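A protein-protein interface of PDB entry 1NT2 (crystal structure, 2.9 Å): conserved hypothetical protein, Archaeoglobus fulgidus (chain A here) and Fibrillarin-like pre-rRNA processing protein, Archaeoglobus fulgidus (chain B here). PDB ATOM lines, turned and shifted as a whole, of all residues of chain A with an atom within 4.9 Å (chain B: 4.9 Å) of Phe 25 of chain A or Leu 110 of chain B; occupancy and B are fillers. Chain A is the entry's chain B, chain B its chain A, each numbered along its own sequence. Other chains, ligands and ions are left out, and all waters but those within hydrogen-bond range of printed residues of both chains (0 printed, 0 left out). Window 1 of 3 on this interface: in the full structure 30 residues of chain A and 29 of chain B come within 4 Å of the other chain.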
ATOM      1  N   TRP A   6       1.481  11.311   1.694  1.00  0.00           N
ATOM      2  CA  TRP A   6       2.013  11.603   0.367  1.00  0.00           C
ATOM      3  C   TRP A   6       2.354  10.425  -0.541  1.00  0.00           C
ATOM      4  O   TRP A   6       2.464  10.603  -1.755  1.00  0.00           O
ATOM      5  CB  TRP A   6       3.233  12.523   0.462  1.00  0.00           C
ATOM      6  CG  TRP A   6       4.488  11.901   1.020  1.00  0.00           C
ATOM      7  CD1 TRP A   6       4.873  11.853   2.333  1.00  0.00           C
ATOM      8  CD2 TRP A   6       5.550  11.301   0.269  1.00  0.00           C
ATOM      9  NE1 TRP A   6       6.111  11.269   2.443  1.00  0.00           N
ATOM     10  CE2 TRP A   6       6.549  10.919   1.193  1.00  0.00           C
ATOM     11  CE3 TRP A   6       5.756  11.051  -1.094  1.00  0.00           C
ATOM     12  CZ2 TRP A   6       7.737  10.300   0.796  1.00  0.00           C
ATOM     13  CZ3 TRP A   6       6.935  10.440  -1.488  1.00  0.00           C
ATOM     14  CH2 TRP A   6       7.913  10.071  -0.544  1.00  0.00           C
ATOM     15  N   PHE A  21       2.945  10.051  -6.995  1.00  0.00           N
ATOM     16  CA  PHE A  21       3.089  10.512  -5.620  1.00  0.00           C
ATOM     17  C   PHE A  21       2.773  11.991  -5.685  1.00  0.00           C
ATOM     18  O   PHE A  21       2.324  12.598  -4.714  1.00  0.00           O
ATOM     19  CB  PHE A  21       4.524  10.311  -5.129  1.00  0.00           C
ATOM     20  CG  PHE A  21       4.913   8.875  -4.988  1.00  0.00           C
ATOM     21  CD1 PHE A  21       6.241   8.501  -5.030  1.00  0.00           C
ATOM     22  CD2 PHE A  21       3.942   7.889  -4.823  1.00  0.00           C
ATOM     23  CE1 PHE A  21       6.602   7.174  -4.916  1.00  0.00           C
ATOM     24  CE2 PHE A  21       4.291   6.558  -4.708  1.00  0.00           C
ATOM     25  CZ  PHE A  21       5.623   6.200  -4.755  1.00  0.00           C
ATOM     26  N   GLU A  22       3.018  12.558  -6.860  1.00  0.00           N
ATOM     27  CA  GLU A  22       2.751  13.957  -7.098  1.00  0.00           C
ATOM     28  C   GLU A  22       1.279  14.219  -6.833  1.00  0.00           C
ATOM     29  O   GLU A  22       0.917  15.254  -6.270  1.00  0.00           O
ATOM     30  CB  GLU A  22       3.099  14.314  -8.539  1.00  0.00           C
ATOM     31  CG  GLU A  22       4.574  14.149  -8.854  1.00  0.00           C
ATOM     32  CD  GLU A  22       4.934  14.617 -10.255  1.00  0.00           C
ATOM     33  OE1 GLU A  22       6.139  14.595 -10.592  1.00  0.00           O
ATOM     34  OE2 GLU A  22       4.019  15.005 -11.017  1.00  0.00           O
ATOM     35  N   GLU A  23       0.430  13.273  -7.221  1.00  0.00           N
ATOM     36  CA  GLU A  23      -0.999  13.442  -7.020  1.00  0.00           C
ATOM     37  C   GLU A  23      -1.362  13.400  -5.550  1.00  0.00           C
ATOM     38  O   GLU A  23      -1.872  14.383  -5.023  1.00  0.00           O
ATOM     39  CB  GLU A  23      -1.785  12.381  -7.784  1.00  0.00           C
ATOM     40  CG  GLU A  23      -2.993  12.951  -8.511  1.00  0.00           C
ATOM     41  CD  GLU A  23      -3.815  11.888  -9.192  1.00  0.00           C
ATOM     42  OE1 GLU A  23      -4.351  11.018  -8.471  1.00  0.00           O
ATOM     43  OE2 GLU A  23      -3.922  11.919 -10.440  1.00  0.00           O
ATOM     44  N   SER A  24      -1.096  12.276  -4.886  1.00  0.00           N
ATOM     45  CA  SER A  24      -1.410  12.136  -3.460  1.00  0.00           C
ATOM     46  C   SER A  24      -0.674  13.170  -2.620  1.00  0.00           C
ATOM     47  O   SER A  24      -1.054  13.446  -1.482  1.00  0.00           O
ATOM     48  CB  SER A  24      -1.049  10.740  -2.957  1.00  0.00           C
ATOM     49  OG  SER A  24       0.318  10.459  -3.197  1.00  0.00           O
ATOM     50  N   PHE A  25       0.393  13.723  -3.183  1.00  0.00           N
ATOM     51  CA  PHE A  25       1.167  14.742  -2.500  1.00  0.00           C
ATOM     52  C   PHE A  25       0.238  15.930  -2.360  1.00  0.00           C
ATOM     53  O   PHE A  25       0.157  16.560  -1.312  1.00  0.00           O
ATOM     54  CB  PHE A  25       2.369  15.147  -3.350  1.00  0.00           C
ATOM     55  CG  PHE A  25       3.332  16.048  -2.641  1.00  0.00           C
ATOM     56  CD1 PHE A  25       4.192  15.539  -1.672  1.00  0.00           C
ATOM     57  CD2 PHE A  25       3.368  17.410  -2.926  1.00  0.00           C
ATOM     58  CE1 PHE A  25       5.074  16.367  -0.996  1.00  0.00           C
ATOM     59  CE2 PHE A  25       4.246  18.249  -2.254  1.00  0.00           C
ATOM     60  CZ  PHE A  25       5.102  17.726  -1.287  1.00  0.00           C
ATOM     61  N   LEU A  26      -0.457  16.222  -3.456  1.00  0.00           N
ATOM     62  CA  LEU A  26      -1.413  17.320  -3.531  1.00  0.00           C
ATOM     63  C   LEU A  26      -2.711  16.892  -2.861  1.00  0.00           C
ATOM     64  O   LEU A  26      -3.564  17.724  -2.541  1.00  0.00           O
ATOM     65  CB  LEU A  26      -1.683  17.671  -4.999  1.00  0.00           C
ATOM     66  CG  LEU A  26      -0.455  18.124  -5.800  1.00  0.00           C
ATOM     67  CD1 LEU A  26      -0.773  18.186  -7.289  1.00  0.00           C
ATOM     68  CD2 LEU A  26       0.004  19.480  -5.284  1.00  0.00           C
ATOM     69  N   LYS A  27      -2.830  15.584  -2.638  1.00  0.00           N
ATOM     70  CA  LYS A  27      -4.018  14.988  -2.031  1.00  0.00           C
ATOM     71  C   LYS A  27      -3.895  14.611  -0.559  1.00  0.00           C
ATOM     72  O   LYS A  27      -4.872  14.162   0.020  1.00  0.00           O
ATOM     73  CB  LYS A  27      -4.440  13.746  -2.829  1.00  0.00           C
ATOM     74  CG  LYS A  27      -4.909  14.057  -4.248  1.00  0.00           C
ATOM     75  CD  LYS A  27      -5.026  12.813  -5.132  1.00  0.00           C
ATOM     76  CE  LYS A  27      -6.105  11.851  -4.669  1.00  0.00           C
ATOM     77  NZ  LYS A  27      -6.218  10.696  -5.598  1.00  0.00           N
ATOM     78  N   ALA A  28      -2.719  14.790   0.042  1.00  0.00           N
ATOM     79  CA  ALA A  28      -2.517  14.452   1.453  1.00  0.00           C
ATOM     80  C   ALA A  28      -3.461  15.210   2.394  1.00  0.00           C
ATOM     81  O   ALA A  28      -3.018  15.961   3.271  1.00  0.00           O
ATOM     82  CB  ALA A  28      -1.082  14.713   1.845  1.00  0.00           C
ATOM     83  N   LEU A  54      10.646  11.822  -1.673  1.00  0.00           N
ATOM     84  CA  LEU A  54       9.767  12.834  -1.074  1.00  0.00           C
ATOM     85  C   LEU A  54      10.158  14.209  -1.598  1.00  0.00           C
ATOM     86  O   LEU A  54       9.333  15.110  -1.689  1.00  0.00           O
ATOM     87  CB  LEU A  54       9.903  12.812   0.457  1.00  0.00           C
ATOM     88  CG  LEU A  54       9.313  13.926   1.324  1.00  0.00           C
ATOM     89  CD1 LEU A  54      10.249  15.083   1.361  1.00  0.00           C
ATOM     90  CD2 LEU A  54       7.962  14.333   0.801  1.00  0.00           C
ATOM     91  N   THR A  57       9.479  14.691  -5.501  1.00  0.00           N
ATOM     92  CA  THR A  57       8.047  14.944  -5.614  1.00  0.00           C
ATOM     93  C   THR A  57       7.728  16.397  -5.291  1.00  0.00           C
ATOM     94  O   THR A  57       7.115  17.100  -6.093  1.00  0.00           O
ATOM     95  CB  THR A  57       7.240  14.047  -4.649  1.00  0.00           C
ATOM     96  OG1 THR A  57       7.681  12.689  -4.783  1.00  0.00           O
ATOM     97  CG2 THR A  57       5.738  14.123  -4.963  1.00  0.00           C
ATOM     98  N   ALA A  58       8.147  16.838  -4.108  1.00  0.00           N
ATOM     99  CA  ALA A  58       7.911  18.205  -3.662  1.00  0.00           C
ATOM    100  C   ALA A  58       8.526  19.208  -4.636  1.00  0.00           C
ATOM    101  O   ALA A  58       8.147  20.378  -4.661  1.00  0.00           O
ATOM    102  CB  ALA A  58       8.488  18.410  -2.253  1.00  0.00           C
ATOM    103  N   VAL A  61       5.973  19.360  -8.250  1.00  0.00           N
ATOM    104  CA  VAL A  61       4.793  20.205  -8.096  1.00  0.00           C
ATOM    105  C   VAL A  61       5.172  21.675  -7.981  1.00  0.00           C
ATOM    106  O   VAL A  61       4.506  22.537  -8.551  1.00  0.00           O
ATOM    107  CB  VAL A  61       3.947  19.813  -6.853  1.00  0.00           C
ATOM    108  CG1 VAL A  61       3.218  18.500  -7.100  1.00  0.00           C
ATOM    109  CG2 VAL A  61       4.831  19.701  -5.640  1.00  0.00           C
ATOM    110  N   TYR B  85      11.203  21.317   5.909  1.00  0.00           N
ATOM    111  CA  TYR B  85       9.956  21.389   5.134  1.00  0.00           C
ATOM    112  C   TYR B  85       9.586  22.864   5.011  1.00  0.00           C
ATOM    113  O   TYR B  85       8.823  23.386   5.820  1.00  0.00           O
ATOM    114  CB  TYR B  85       8.805  20.643   5.835  1.00  0.00           C
ATOM    115  CG  TYR B  85       8.999  19.146   6.034  1.00  0.00           C
ATOM    116  CD1 TYR B  85       9.503  18.641   7.229  1.00  0.00           C
ATOM    117  CD2 TYR B  85       8.652  18.236   5.037  1.00  0.00           C
ATOM    118  CE1 TYR B  85       9.652  17.269   7.427  1.00  0.00           C
ATOM    119  CE2 TYR B  85       8.799  16.865   5.227  1.00  0.00           C
ATOM    120  CZ  TYR B  85       9.299  16.391   6.425  1.00  0.00           C
ATOM    121  OH  TYR B  85       9.439  15.034   6.631  1.00  0.00           O
ATOM    122  N   ALA B  86      10.125  23.535   4.002  1.00  0.00           N
ATOM    123  CA  ALA B  86       9.857  24.953   3.833  1.00  0.00           C
ATOM    124  C   ALA B  86       8.567  25.238   3.076  1.00  0.00           C
ATOM    125  O   ALA B  86       8.401  24.795   1.943  1.00  0.00           O
ATOM    126  CB  ALA B  86      11.028  25.603   3.134  1.00  0.00           C
ATOM    127  N   VAL B  87       7.662  25.984   3.713  1.00  0.00           N
ATOM    128  CA  VAL B  87       6.372  26.347   3.109  1.00  0.00           C
ATOM    129  C   VAL B  87       6.278  27.842   2.756  1.00  0.00           C
ATOM    130  O   VAL B  87       6.612  28.706   3.568  1.00  0.00           O
ATOM    131  CB  VAL B  87       5.183  25.993   4.043  1.00  0.00           C
ATOM    132  CG1 VAL B  87       5.344  24.579   4.577  1.00  0.00           C
ATOM    133  CG2 VAL B  87       5.085  26.993   5.175  1.00  0.00           C
ATOM    134  N   GLU B  88       5.819  28.131   1.538  1.00  0.00           N
ATOM    135  CA  GLU B  88       5.666  29.500   1.041  1.00  0.00           C
ATOM    136  C   GLU B  88       4.582  29.455  -0.030  1.00  0.00           C
ATOM    137  O   GLU B  88       4.668  28.649  -0.953  1.00  0.00           O
ATOM    138  CB  GLU B  88       6.985  29.981   0.433  1.00  0.00           C
ATOM    139  CG  GLU B  88       6.873  31.262  -0.358  1.00  0.00           C
ATOM    140  CD  GLU B  88       6.352  32.418   0.467  1.00  0.00           C
ATOM    141  OE1 GLU B  88       7.084  32.907   1.354  1.00  0.00           O
ATOM    142  OE2 GLU B  88       5.202  32.831   0.228  1.00  0.00           O
ATOM    143  N   PHE B  94       8.830  32.184  -4.357  1.00  0.00           N
ATOM    144  CA  PHE B  94       8.986  30.751  -4.479  1.00  0.00           C
ATOM    145  C   PHE B  94       9.827  30.406  -5.690  1.00  0.00           C
ATOM    146  O   PHE B  94      10.594  29.456  -5.660  1.00  0.00           O
ATOM    147  CB  PHE B  94       7.616  30.083  -4.595  1.00  0.00           C
ATOM    148  CG  PHE B  94       7.610  28.654  -4.163  1.00  0.00           C
ATOM    149  CD1 PHE B  94       7.528  28.326  -2.814  1.00  0.00           C
ATOM    150  CD2 PHE B  94       7.769  27.634  -5.097  1.00  0.00           C
ATOM    151  CE1 PHE B  94       7.610  27.001  -2.398  1.00  0.00           C
ATOM    152  CE2 PHE B  94       7.854  26.309  -4.694  1.00  0.00           C
ATOM    153  CZ  PHE B  94       7.776  25.990  -3.341  1.00  0.00           C
ATOM    154  N   ILE B 108      12.752  20.558   1.673  1.00  0.00           N
ATOM    155  CA  ILE B 108      11.542  20.078   1.012  1.00  0.00           C
ATOM    156  C   ILE B 108      10.545  21.225   0.814  1.00  0.00           C
ATOM    157  O   ILE B 108      10.050  21.820   1.780  1.00  0.00           O
ATOM    158  CB  ILE B 108      10.857  18.983   1.845  1.00  0.00           C
ATOM    159  CG1 ILE B 108      11.863  17.875   2.196  1.00  0.00           C
ATOM    160  CG2 ILE B 108       9.661  18.438   1.075  1.00  0.00           C
ATOM    161  CD1 ILE B 108      12.470  17.165   0.990  1.00  0.00           C
ATOM    162  N   PRO B 109      10.229  21.537  -0.454  1.00  0.00           N
ATOM    163  CA  PRO B 109       9.306  22.609  -0.824  1.00  0.00           C
ATOM    164  C   PRO B 109       7.824  22.295  -0.713  1.00  0.00           C
ATOM    165  O   PRO B 109       7.327  21.328  -1.273  1.00  0.00           O
ATOM    166  CB  PRO B 109       9.725  22.925  -2.249  1.00  0.00           C
ATOM    167  CG  PRO B 109      10.057  21.571  -2.781  1.00  0.00           C
ATOM    168  CD  PRO B 109      10.830  20.923  -1.655  1.00  0.00           C
ATOM    169  N   LEU B 110       7.129  23.139   0.035  1.00  0.00           N
ATOM    170  CA  LEU B 110       5.693  23.016   0.238  1.00  0.00           C
ATOM    171  C   LEU B 110       5.097  24.348  -0.184  1.00  0.00           C
ATOM    172  O   LEU B 110       5.116  25.328   0.559  1.00  0.00           O
ATOM    173  CB  LEU B 110       5.367  22.729   1.707  1.00  0.00           C
ATOM    174  CG  LEU B 110       6.024  21.487   2.336  1.00  0.00           C
ATOM    175  CD1 LEU B 110       5.349  21.173   3.680  1.00  0.00           C
ATOM    176  CD2 LEU B 110       5.912  20.288   1.394  1.00  0.00           C
ATOM    177  N   LEU B 111       4.590  24.357  -1.403  1.00  0.00           N
ATOM    178  CA  LEU B 111       3.984  25.510  -2.034  1.00  0.00           C
ATOM    179  C   LEU B 111       2.515  25.664  -1.657  1.00  0.00           C
ATOM    180  O   LEU B 111       1.672  25.950  -2.513  1.00  0.00           O
ATOM    181  CB  LEU B 111       4.114  25.331  -3.534  1.00  0.00           C
ATOM    182  CG  LEU B 111       4.134  23.852  -3.947  1.00  0.00           C
ATOM    183  CD1 LEU B 111       5.420  23.184  -3.455  1.00  0.00           C
ATOM    184  CD2 LEU B 111       2.918  23.138  -3.386  1.00  0.00           C
ATOM    185  N   PHE B 112       2.225  25.488  -0.370  1.00  0.00           N
ATOM    186  CA  PHE B 112       0.863  25.567   0.149  1.00  0.00           C
ATOM    187  C   PHE B 112       0.663  26.664   1.166  1.00  0.00           C
ATOM    188  O   PHE B 112       1.621  27.179   1.731  1.00  0.00           O
ATOM    189  CB  PHE B 112       0.492  24.246   0.796  1.00  0.00           C
ATOM    190  CG  PHE B 112       0.715  23.069  -0.084  1.00  0.00           C
ATOM    191  CD1 PHE B 112      -0.044  22.895  -1.235  1.00  0.00           C
ATOM    192  CD2 PHE B 112       1.679  22.129   0.233  1.00  0.00           C
ATOM    193  CE1 PHE B 112       0.151  21.790  -2.065  1.00  0.00           C
ATOM    194  CE2 PHE B 112       1.886  21.016  -0.588  1.00  0.00           C
ATOM    195  CZ  PHE B 112       1.117  20.847  -1.743  1.00  0.00           C
ATOM    196  N   TYR B 120      -1.658  20.019   4.261  1.00  0.00           N
ATOM    197  CA  TYR B 120      -0.419  19.315   3.929  1.00  0.00           C
ATOM    198  C   TYR B 120       0.014  18.387   5.081  1.00  0.00           C
ATOM    199  O   TYR B 120       1.132  17.858   5.103  1.00  0.00           O
ATOM    200  CB  TYR B 120       0.690  20.334   3.578  1.00  0.00           C
ATOM    201  CG  TYR B 120       0.965  21.381   4.643  1.00  0.00           C
ATOM    202  CD1 TYR B 120       1.566  21.032   5.853  1.00  0.00           C
ATOM    203  CD2 TYR B 120       0.585  22.708   4.462  1.00  0.00           C
ATOM    204  CE1 TYR B 120       1.774  21.976   6.857  1.00  0.00           C
ATOM    205  CE2 TYR B 120       0.792  23.658   5.462  1.00  0.00           C
ATOM    206  CZ  TYR B 120       1.387  23.285   6.656  1.00  0.00           C
ATOM    207  OH  TYR B 120       1.596  24.212   7.650  1.00  0.00           O
ATOM    208  N   ILE B 123       2.165  15.225   4.803  1.00  0.00           N
ATOM    209  CA  ILE B 123       3.494  15.349   4.207  1.00  0.00           C
ATOM    210  C   ILE B 123       4.500  15.671   5.297  1.00  0.00           C
ATOM    211  O   ILE B 123       5.609  15.132   5.334  1.00  0.00           O
ATOM    212  CB  ILE B 123       3.550  16.498   3.160  1.00  0.00           C
ATOM    213  CG1 ILE B 123       2.580  16.226   2.009  1.00  0.00           C
ATOM    214  CG2 ILE B 123       4.966  16.640   2.619  1.00  0.00           C
ATOM    215  CD1 ILE B 123       2.568  17.308   0.953  1.00  0.00           C
ATOM    216  N   VAL B 124       4.108  16.568   6.185  1.00  0.00           N
ATOM    217  CA  VAL B 124       4.985  16.964   7.264  1.00  0.00           C
ATOM    218  C   VAL B 124       4.956  15.923   8.371  1.00  0.00           C
ATOM    219  O   VAL B 124       3.890  15.473   8.786  1.00  0.00           O
ATOM    220  CB  VAL B 124       4.568  18.333   7.823  1.00  0.00           C
ATOM    221  CG1 VAL B 124       5.508  18.756   8.927  1.00  0.00           C
ATOM    222  CG2 VAL B 124       4.567  19.354   6.700  1.00  0.00           C
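CZ of Phe 25 of chain A touches CD2 of Leu 110 of chain B, at 3.8 Å. CE1 of Phe 25 of chain A touches CD1 of Ile 123 of chain B (3.3 Å). Phe 112 of chain B touches Leu 26 of chain A (CZ to CD2, 3.96 Å). Ala 28 of chain A touches Ile 123 of chain B. CD1 of Leu 54 of chain A touches CD1 of Ile 108 of chain B, at 3.1 Å. Ile 108 of chain B touches Ala 58 of chain A (CG2 to CB, 3.5 Å). CG of Pro 109 of chain B touches O of Ala 58 of chain A, 2.9 Å away.
Printed residues of chain A that touch a printed residue of chain B: Phe 25, Leu 26, Ala 28, Leu 54 and Ala 58. Of the 13 printed residues of chain B, 5 touch a printed residue of chain A.
Printed residues of chain B within 4 Å of Ala 28 of chain A: Ile 123. Of the printed residues of chain A, Ile 108 of chain B touches Leu 54 (3.1 Å) and Ala 58 (3.5 Å). Of the printed residues of chain A, Leu 110 of chain B touches Phe 25. The nearest residue of chain A that does not touch Leu 110 of chain B is Ala 58 of chain A (4.8 Å).
The backbone NH (N) of Glu 88 of chain B lies within hydrogen-bond range of the backbone carbonyl oxygen (O) of Leu 110 of chain B, at 3.1 Å. The backbone NH (N) of Leu 110 of chain B is in hydrogen-bond range of the backbone carbonyl oxygen (O) of Ala 86 of chain B (2.8 Å). The backbone NH (N) of Ala 86 of chain B sits at hydrogen-bond distance from the backbone carbonyl oxygen (O) of Ile 108 of chain B.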
